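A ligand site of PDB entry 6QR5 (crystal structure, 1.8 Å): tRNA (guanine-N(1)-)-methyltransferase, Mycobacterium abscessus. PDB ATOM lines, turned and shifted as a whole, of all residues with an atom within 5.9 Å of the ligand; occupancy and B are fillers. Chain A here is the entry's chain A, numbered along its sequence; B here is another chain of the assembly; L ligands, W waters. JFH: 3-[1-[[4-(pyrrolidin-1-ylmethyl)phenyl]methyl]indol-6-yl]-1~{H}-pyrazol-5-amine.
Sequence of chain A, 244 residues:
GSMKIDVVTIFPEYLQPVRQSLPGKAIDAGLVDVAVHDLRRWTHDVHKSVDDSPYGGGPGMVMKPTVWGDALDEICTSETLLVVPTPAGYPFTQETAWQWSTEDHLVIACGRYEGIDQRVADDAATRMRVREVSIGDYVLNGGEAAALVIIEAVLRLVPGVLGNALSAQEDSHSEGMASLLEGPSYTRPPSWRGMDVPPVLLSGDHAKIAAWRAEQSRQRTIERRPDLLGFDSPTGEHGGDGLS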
ATOM      1  N   PRO A  85     -11.794  13.160 -21.717  1.00  0.00           N
ATOM      2  CA  PRO A  85     -13.069  13.101 -20.993  1.00  0.00           C
ATOM      3  C   PRO A  85     -12.925  13.551 -19.547  1.00  0.00           C
ATOM      4  O   PRO A  85     -11.926  13.260 -18.888  1.00  0.00           O
ATOM      5  CB  PRO A  85     -13.454  11.629 -21.094  1.00  0.00           C
ATOM      6  CG  PRO A  85     -12.770  11.156 -22.376  1.00  0.00           C
ATOM      7  CD  PRO A  85     -11.454  11.875 -22.345  1.00  0.00           C
ATOM      8  N   THR A  86     -13.936  14.265 -19.061  1.00  0.00           N
ATOM      9  CA  THR A  86     -13.932  14.752 -17.679  1.00  0.00           C
ATOM     10  C   THR A  86     -15.345  15.246 -17.358  1.00  0.00           C
ATOM     11  O   THR A  86     -16.003  15.805 -18.234  1.00  0.00           O
ATOM     12  CB  THR A  86     -12.895  15.885 -17.458  1.00  0.00           C
ATOM     13  OG1 THR A  86     -13.190  16.573 -16.233  1.00  0.00           O
ATOM     14  CG2 THR A  86     -12.870  16.880 -18.616  1.00  0.00           C
ATOM     15  N   PRO A  87     -15.809  15.034 -16.122  1.00  0.00           N
ATOM     16  CA  PRO A  87     -17.127  15.530 -15.706  1.00  0.00           C
ATOM     17  C   PRO A  87     -17.193  17.040 -15.782  1.00  0.00           C
ATOM     18  O   PRO A  87     -18.277  17.599 -15.844  1.00  0.00           O
ATOM     19  CB  PRO A  87     -17.254  15.065 -14.250  1.00  0.00           C
ATOM     20  CG  PRO A  87     -16.201  14.083 -14.036  1.00  0.00           C
ATOM     21  CD  PRO A  87     -15.094  14.378 -15.018  1.00  0.00           C
ATOM     22  N   CYS A 110      -7.804   8.741 -21.297  1.00  0.00           N
ATOM     23  CA  CYS A 110      -8.795   8.303 -20.308  1.00  0.00           C
ATOM     24  C   CYS A 110      -8.231   8.356 -18.900  1.00  0.00           C
ATOM     25  O   CYS A 110      -7.289   7.627 -18.577  1.00  0.00           O
ATOM     26  CB  CYS A 110      -9.267   6.876 -20.594  1.00  0.00           C
ATOM     27  SG  CYS A 110     -10.076   6.647 -22.200  1.00  0.00           S
ATOM     28  N   GLY A 111      -8.805   9.226 -18.083  1.00  0.00           N
ATOM     29  CA  GLY A 111      -8.447   9.307 -16.683  1.00  0.00           C
ATOM     30  C   GLY A 111      -9.136   8.256 -15.822  1.00  0.00           C
ATOM     31  O   GLY A 111     -10.161   7.664 -16.207  1.00  0.00           O
ATOM     32  N   ARG A 112      -8.543   8.021 -14.665  1.00  0.00           N
ATOM     33  CA  ARG A 112      -9.192   7.245 -13.617  1.00  0.00           C
ATOM     34  C   ARG A 112      -8.971   7.989 -12.307  1.00  0.00           C
ATOM     35  O   ARG A 112      -8.550   9.149 -12.325  1.00  0.00           O
ATOM     36  CB  ARG A 112      -8.667   5.811 -13.554  1.00  0.00           C
ATOM     37  CG  ARG A 112      -9.295   4.890 -14.581  1.00  0.00           C
ATOM     38  CD  ARG A 112     -10.550   4.201 -14.031  1.00  0.00           C
ATOM     39  NE  ARG A 112     -11.431   3.711 -15.091  1.00  0.00           N
ATOM     40  CZ  ARG A 112     -12.483   2.941 -14.896  1.00  0.00           C
ATOM     41  NH1 ARG A 112     -12.782   2.514 -13.667  1.00  0.00           N
ATOM     42  NH2 ARG A 112     -13.238   2.560 -15.926  1.00  0.00           N
ATOM     43  N   TYR A 113      -9.247   7.331 -11.182  1.00  0.00           N
ATOM     44  CA  TYR A 113      -9.145   7.975  -9.878  1.00  0.00           C
ATOM     45  C   TYR A 113     -10.004   9.226  -9.928  1.00  0.00           C
ATOM     46  O   TYR A 113     -11.158   9.150 -10.338  1.00  0.00           O
ATOM     47  CB  TYR A 113      -7.675   8.274  -9.528  1.00  0.00           C
ATOM     48  CG  TYR A 113      -6.829   7.018  -9.645  1.00  0.00           C
ATOM     49  CD1 TYR A 113      -6.225   6.684 -10.849  1.00  0.00           C
ATOM     50  CD2 TYR A 113      -6.683   6.143  -8.575  1.00  0.00           C
ATOM     51  CE1 TYR A 113      -5.480   5.518 -10.974  1.00  0.00           C
ATOM     52  CE2 TYR A 113      -5.921   4.988  -8.686  1.00  0.00           C
ATOM     53  CZ  TYR A 113      -5.329   4.680  -9.888  1.00  0.00           C
ATOM     54  OH  TYR A 113      -4.572   3.529 -10.030  1.00  0.00           O
ATOM     55  N   GLU A 114      -9.491  10.379  -9.527  1.00  0.00           N
ATOM     56  CA  GLU A 114     -10.309  11.586  -9.620  1.00  0.00           C
ATOM     57  C   GLU A 114      -9.863  12.556 -10.713  1.00  0.00           C
ATOM     58  O   GLU A 114     -10.239  13.720 -10.718  1.00  0.00           O
ATOM     59  CB  GLU A 114     -10.339  12.288  -8.272  1.00  0.00           C
ATOM     60  CG  GLU A 114     -10.854  11.363  -7.166  1.00  0.00           C
ATOM     61  CD  GLU A 114     -12.027  11.932  -6.407  1.00  0.00           C
ATOM     62  OE1 GLU A 114     -12.784  11.142  -5.820  1.00  0.00           O
ATOM     63  OE2 GLU A 114     -12.179  13.176  -6.378  1.00  0.00           O
ATOM     64  N   GLY A 115      -9.077  12.060 -11.659  1.00  0.00           N
ATOM     65  CA  GLY A 115      -8.741  12.861 -12.821  1.00  0.00           C
ATOM     66  C   GLY A 115      -7.245  12.965 -13.044  1.00  0.00           C
ATOM     67  O   GLY A 115      -6.468  12.306 -12.373  1.00  0.00           O
ATOM     68  N   VAL A 133     -13.907  17.275 -22.475  1.00  0.00           N
ATOM     69  CA  VAL A 133     -15.335  17.161 -22.755  1.00  0.00           C
ATOM     70  C   VAL A 133     -16.057  16.242 -21.789  1.00  0.00           C
ATOM     71  O   VAL A 133     -15.467  15.294 -21.270  1.00  0.00           O
ATOM     72  CB  VAL A 133     -15.602  16.655 -24.196  1.00  0.00           C
ATOM     73  CG1 VAL A 133     -15.220  17.712 -25.214  1.00  0.00           C
ATOM     74  CG2 VAL A 133     -14.833  15.358 -24.470  1.00  0.00           C
ATOM     75  N   SER A 134     -17.332  16.555 -21.556  1.00  0.00           N
ATOM     76  CA  SER A 134     -18.211  15.736 -20.734  1.00  0.00           C
ATOM     77  C   SER A 134     -19.244  15.125 -21.665  1.00  0.00           C
ATOM     78  O   SER A 134     -19.737  15.815 -22.568  1.00  0.00           O
ATOM     79  CB  SER A 134     -18.912  16.582 -19.657  1.00  0.00           C
ATOM     80  OG  SER A 134     -19.945  15.841 -19.033  1.00  0.00           O
ATOM     81  N   ILE A 135     -19.613  13.868 -21.441  1.00  0.00           N
ATOM     82  CA  ILE A 135     -20.665  13.266 -22.267  1.00  0.00           C
ATOM     83  C   ILE A 135     -22.065  13.308 -21.634  1.00  0.00           C
ATOM     84  O   ILE A 135     -23.044  12.817 -22.218  1.00  0.00           O
ATOM     85  CB  ILE A 135     -20.349  11.805 -22.623  1.00  0.00           C
ATOM     86  CG1 ILE A 135     -20.223  10.947 -21.358  1.00  0.00           C
ATOM     87  CG2 ILE A 135     -19.076  11.720 -23.499  1.00  0.00           C
ATOM     88  CD1 ILE A 135     -20.491   9.436 -21.615  1.00  0.00           C
ATOM     89  N   GLY A 136     -22.170  13.912 -20.446  1.00  0.00           N
ATOM     90  CA  GLY A 136     -23.463  14.081 -19.805  1.00  0.00           C
ATOM     91  C   GLY A 136     -23.294  14.436 -18.349  1.00  0.00           C
ATOM     92  O   GLY A 136     -22.207  14.352 -17.799  1.00  0.00           O
ATOM     93  N   ASP A 137     -24.385  14.839 -17.713  1.00  0.00           N
ATOM     94  CA  ASP A 137     -24.317  15.347 -16.358  1.00  0.00           C
ATOM     95  C   ASP A 137     -24.483  14.254 -15.325  1.00  0.00           C
ATOM     96  O   ASP A 137     -25.411  14.276 -14.496  1.00  0.00           O
ATOM     97  CB  ASP A 137     -25.377  16.442 -16.149  1.00  0.00           C
ATOM     98  CG  ASP A 137     -25.088  17.675 -16.950  1.00  0.00           C
ATOM     99  OD1 ASP A 137     -23.905  17.870 -17.333  1.00  0.00           O
ATOM    100  OD2 ASP A 137     -26.022  18.454 -17.207  1.00  0.00           O
ATOM    101  N   TYR A 138     -23.593  13.278 -15.406  1.00  0.00           N
ATOM    102  CA  TYR A 138     -23.491  12.197 -14.438  1.00  0.00           C
ATOM    103  C   TYR A 138     -22.010  11.898 -14.302  1.00  0.00           C
ATOM    104  O   TYR A 138     -21.214  12.279 -15.162  1.00  0.00           O
ATOM    105  CB  TYR A 138     -24.269  10.964 -14.915  1.00  0.00           C
ATOM    106  CG  TYR A 138     -24.098  10.748 -16.394  1.00  0.00           C
ATOM    107  CD1 TYR A 138     -22.932  10.168 -16.904  1.00  0.00           C
ATOM    108  CD2 TYR A 138     -25.078  11.179 -17.288  1.00  0.00           C
ATOM    109  CE1 TYR A 138     -22.754  10.006 -18.271  1.00  0.00           C
ATOM    110  CE2 TYR A 138     -24.918  11.018 -18.642  1.00  0.00           C
ATOM    111  CZ  TYR A 138     -23.760  10.434 -19.132  1.00  0.00           C
ATOM    112  OH  TYR A 138     -23.606  10.285 -20.481  1.00  0.00           O
ATOM    113  N   VAL A 139     -21.652  11.216 -13.234  1.00  0.00           N
ATOM    114  CA  VAL A 139     -20.255  10.907 -12.966  1.00  0.00           C
ATOM    115  C   VAL A 139     -19.961   9.443 -13.212  1.00  0.00           C
ATOM    116  O   VAL A 139     -20.653   8.557 -12.683  1.00  0.00           O
ATOM    117  CB  VAL A 139     -19.884  11.261 -11.511  1.00  0.00           C
ATOM    118  CG1 VAL A 139     -18.418  10.903 -11.248  1.00  0.00           C
ATOM    119  CG2 VAL A 139     -20.139  12.735 -11.241  1.00  0.00           C
ATOM    120  N   LEU A 140     -18.949   9.171 -14.026  1.00  0.00           N
ATOM    121  CA  LEU A 140     -18.511   7.818 -14.318  1.00  0.00           C
ATOM    122  C   LEU A 140     -17.356   7.473 -13.383  1.00  0.00           C
ATOM    123  O   LEU A 140     -16.964   8.289 -12.567  1.00  0.00           O
ATOM    124  CB  LEU A 140     -18.082   7.702 -15.787  1.00  0.00           C
ATOM    125  CG  LEU A 140     -19.130   8.056 -16.844  1.00  0.00           C
ATOM    126  CD1 LEU A 140     -18.493   8.289 -18.212  1.00  0.00           C
ATOM    127  CD2 LEU A 140     -20.181   6.962 -16.926  1.00  0.00           C
ATOM    128  N   ASN A 141     -16.796   6.274 -13.525  1.00  0.00           N
ATOM    129  CA  ASN A 141     -15.619   5.887 -12.731  1.00  0.00           C
ATOM    130  C   ASN A 141     -14.297   6.313 -13.381  1.00  0.00           C
ATOM    131  O   ASN A 141     -13.223   6.269 -12.747  1.00  0.00           O
ATOM    132  CB  ASN A 141     -15.598   4.380 -12.509  1.00  0.00           C
ATOM    133  CG  ASN A 141     -16.348   3.970 -11.269  1.00  0.00           C
ATOM    134  OD1 ASN A 141     -16.349   4.681 -10.270  1.00  0.00           O
ATOM    135  ND2 ASN A 141     -16.991   2.809 -11.338  1.00  0.00           N
ATOM    136  N   GLY A 142     -14.387   6.715 -14.645  1.00  0.00           N
ATOM    137  CA  GLY A 142     -13.204   7.051 -15.415  1.00  0.00           C
ATOM    138  C   GLY A 142     -13.571   7.392 -16.844  1.00  0.00           C
ATOM    139  O   GLY A 142     -14.747   7.354 -17.214  1.00  0.00           O
ATOM    140  N   GLY A 143     -12.587   7.705 -17.669  1.00  0.00           N
ATOM    141  CA  GLY A 143     -12.847   8.169 -19.026  1.00  0.00           C
ATOM    142  C   GLY A 143     -13.220   7.110 -20.052  1.00  0.00           C
ATOM    143  O   GLY A 143     -13.687   7.462 -21.141  1.00  0.00           O
ATOM    144  N   ALA A 146     -16.714   6.967 -21.483  1.00  0.00           N
ATOM    145  CA  ALA A 146     -16.890   8.179 -22.279  1.00  0.00           C
ATOM    146  C   ALA A 146     -16.193   8.053 -23.625  1.00  0.00           C
ATOM    147  O   ALA A 146     -16.709   8.514 -24.651  1.00  0.00           O
ATOM    148  CB  ALA A 146     -16.381   9.407 -21.536  1.00  0.00           C
ATOM    149  N   ARG B 156     -21.586   2.869  -9.017  1.00  0.00           N
ATOM    150  CA  ARG B 156     -20.608   3.524  -8.162  1.00  0.00           C
ATOM    151  C   ARG B 156     -21.312   4.246  -7.009  1.00  0.00           C
ATOM    152  O   ARG B 156     -20.654   4.714  -6.067  1.00  0.00           O
ATOM    153  CB  ARG B 156     -19.731   4.469  -8.982  1.00  0.00           C
ATOM    154  CG  ARG B 156     -20.456   5.607  -9.628  1.00  0.00           C
ATOM    155  CD  ARG B 156     -19.481   6.454 -10.443  1.00  0.00           C
ATOM    156  NE  ARG B 156     -18.488   7.130  -9.601  1.00  0.00           N
ATOM    157  CZ  ARG B 156     -18.721   8.243  -8.913  1.00  0.00           C
ATOM    158  NH1 ARG B 156     -19.923   8.808  -8.933  1.00  0.00           N
ATOM    159  NH2 ARG B 156     -17.759   8.801  -8.199  1.00  0.00           N
ATOM    160  N   LEU B 180     -22.254  22.136  -9.945  1.00  0.00           N
ATOM    161  CA  LEU B 180     -21.070  22.890 -10.363  1.00  0.00           C
ATOM    162  C   LEU B 180     -20.011  21.961 -10.959  1.00  0.00           C
ATOM    163  O   LEU B 180     -20.005  20.773 -10.680  1.00  0.00           O
ATOM    164  CB  LEU B 180     -20.464  23.655  -9.196  1.00  0.00           C
ATOM    165  CG  LEU B 180     -21.261  24.813  -8.622  1.00  0.00           C
ATOM    166  CD1 LEU B 180     -20.548  25.348  -7.400  1.00  0.00           C
ATOM    167  CD2 LEU B 180     -21.450  25.901  -9.660  1.00  0.00           C
ATOM    168  N   GLU B 182     -16.196  20.616 -11.213  1.00  0.00           N
ATOM    169  CA  GLU B 182     -14.999  20.556 -10.362  1.00  0.00           C
ATOM    170  C   GLU B 182     -13.847  21.316 -11.006  1.00  0.00           C
ATOM    171  O   GLU B 182     -13.699  21.338 -12.233  1.00  0.00           O
ATOM    172  CB  GLU B 182     -14.601  19.097 -10.094  1.00  0.00           C
HETATM  173  C10 JFH L   1     -13.747  10.374 -14.475  1.00  0.00           C
HETATM  174  C13 JFH L   1     -14.250  10.806 -11.147  1.00  0.00           C
HETATM  175  C15 JFH L   1     -14.024  13.137 -10.541  1.00  0.00           C
HETATM  176  C17 JFH L   1     -15.000  13.999  -8.290  1.00  0.00           C
HETATM  177  C20 JFH L   1     -17.977  15.521  -9.001  1.00  0.00           C
HETATM  178  C21 JFH L   1     -17.587  15.932  -7.916  1.00  0.00           C
HETATM  179  C22 JFH L   1     -15.991  15.767  -7.902  1.00  0.00           C
HETATM  180  C24 JFH L   1     -14.929  10.549  -9.952  1.00  0.00           C
HETATM  181  C26 JFH L   1     -11.517  10.174 -14.600  1.00  0.00           C
HETATM  182  C28 JFH L   1     -17.107  12.195 -17.698  1.00  0.00           C
HETATM  183  C02 JFH L   1     -18.489  12.348 -17.586  1.00  0.00           C
HETATM  184  C05 JFH L   1     -16.715  11.447 -16.617  1.00  0.00           C
HETATM  185  C06 JFH L   1     -15.308  11.094 -16.228  1.00  0.00           C
HETATM  186  C07 JFH L   1     -14.250  11.272 -17.106  1.00  0.00           C
HETATM  187  C08 JFH L   1     -12.942  10.993 -16.689  1.00  0.00           C
HETATM  188  C09 JFH L   1     -12.701  10.539 -15.337  1.00  0.00           C
HETATM  189  C12 JFH L   1     -14.037   9.631 -12.103  1.00  0.00           C
HETATM  190  C14 JFH L   1     -13.806  12.114 -11.451  1.00  0.00           C
HETATM  191  C16 JFH L   1     -14.715  12.869  -9.339  1.00  0.00           C
HETATM  192  C19 JFH L   1     -16.953  14.464  -9.400  1.00  0.00           C
HETATM  193  C23 JFH L   1     -15.156  11.574  -9.040  1.00  0.00           C
HETATM  194  C25 JFH L   1     -11.926   9.807 -13.326  1.00  0.00           C
HETATM  195  C27 JFH L   1     -15.074  10.664 -14.897  1.00  0.00           C
HETATM  196  N01 JFH L   1     -19.350  13.023 -18.487  1.00  0.00           N
HETATM  197  N03 JFH L   1     -18.870  11.743 -16.432  1.00  0.00           N
HETATM  198  N04 JFH L   1     -17.777  11.228 -15.856  1.00  0.00           N
HETATM  199  N11 JFH L   1     -13.248   9.943 -13.258  1.00  0.00           N
HETATM  200  N18 JFH L   1     -15.668  14.921  -8.783  1.00  0.00           N
HETATM  201  O   HOH W   1     -11.861  13.660 -14.640  1.00  0.00           O
HETATM  202  O   HOH W   2     -15.121   7.780  -8.013  1.00  0.00           O
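A nitrogen (N01) of the ligand sits at hydrogen-bond distance from the side-chain hydroxyl (OG) of Ser 134, at 2.9 Å.
N04 of the ligand is in hydrogen-bond range of N of Leu 140 (3.0 Å).
N01 of the ligand is in hydrogen-bond range of O of Gly 136 (3.2 Å).
O of Tyr 138 lies within hydrogen-bond range of N03 of the ligand (2.7 Å).
The backbone carbonyl oxygen (O) of Gly 136 is in hydrogen-bond range of the side-chain hydroxyl (OG) of Ser 134, 3.0 Å away.
OD1 of Asn 141 lies within hydrogen-bond range of NE of Arg 156 of chain B (3.3 Å).
The side-chain hydroxyl of Tyr 138 sits at hydrogen-bond distance from the backbone carbonyl oxygen of Ile 135, at 3.1 Å.
N of Gly 143 lies within hydrogen-bond range of O of Gly 111 (2.8 Å).
O of Val 133 is in hydrogen-bond range of N of Thr 86 (2.9 Å).
The backbone NH of Ile 135 lies close to a nitrogen (N01) of the ligand, at 3.1 Å.
Pro 85 touches the ligand.
Thr 86 touches the ligand (C to C28, 3.5 Å).
Pro 87 touches the ligand (N to C28, 3.5 Å).
Gly 111 touches the ligand.
O of Arg 112 touches C25 of the ligand, at 3.6 Å.
O of Tyr 113 touches C25 of the ligand, at 3.2 Å.
OE2 of Glu 114 touches C17 of the ligand, 3.5 Å away.
Gly 115 touches the ligand.
CG1 of Val 139 touches C24 of the ligand, 3.7 Å away.
Asn 141 touches the ligand (O to C12, 3.5 Å).
CA of Gly 142 touches C10 of the ligand (3.5 Å).
N of Gly 143 touches C08 of the ligand, at 3.4 Å.
Arg 156 of chain B touches the ligand.
Hydrophobic or aromatic side chains that line the ligand: Pro 87, Ile 135, Val 139 and Leu 140.
Of the 24 residues printed, 18 come within 4 Å of the ligand.
The nearest printed residue that does not touch the ligand is Glu 182 of chain B (4.2 Å).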
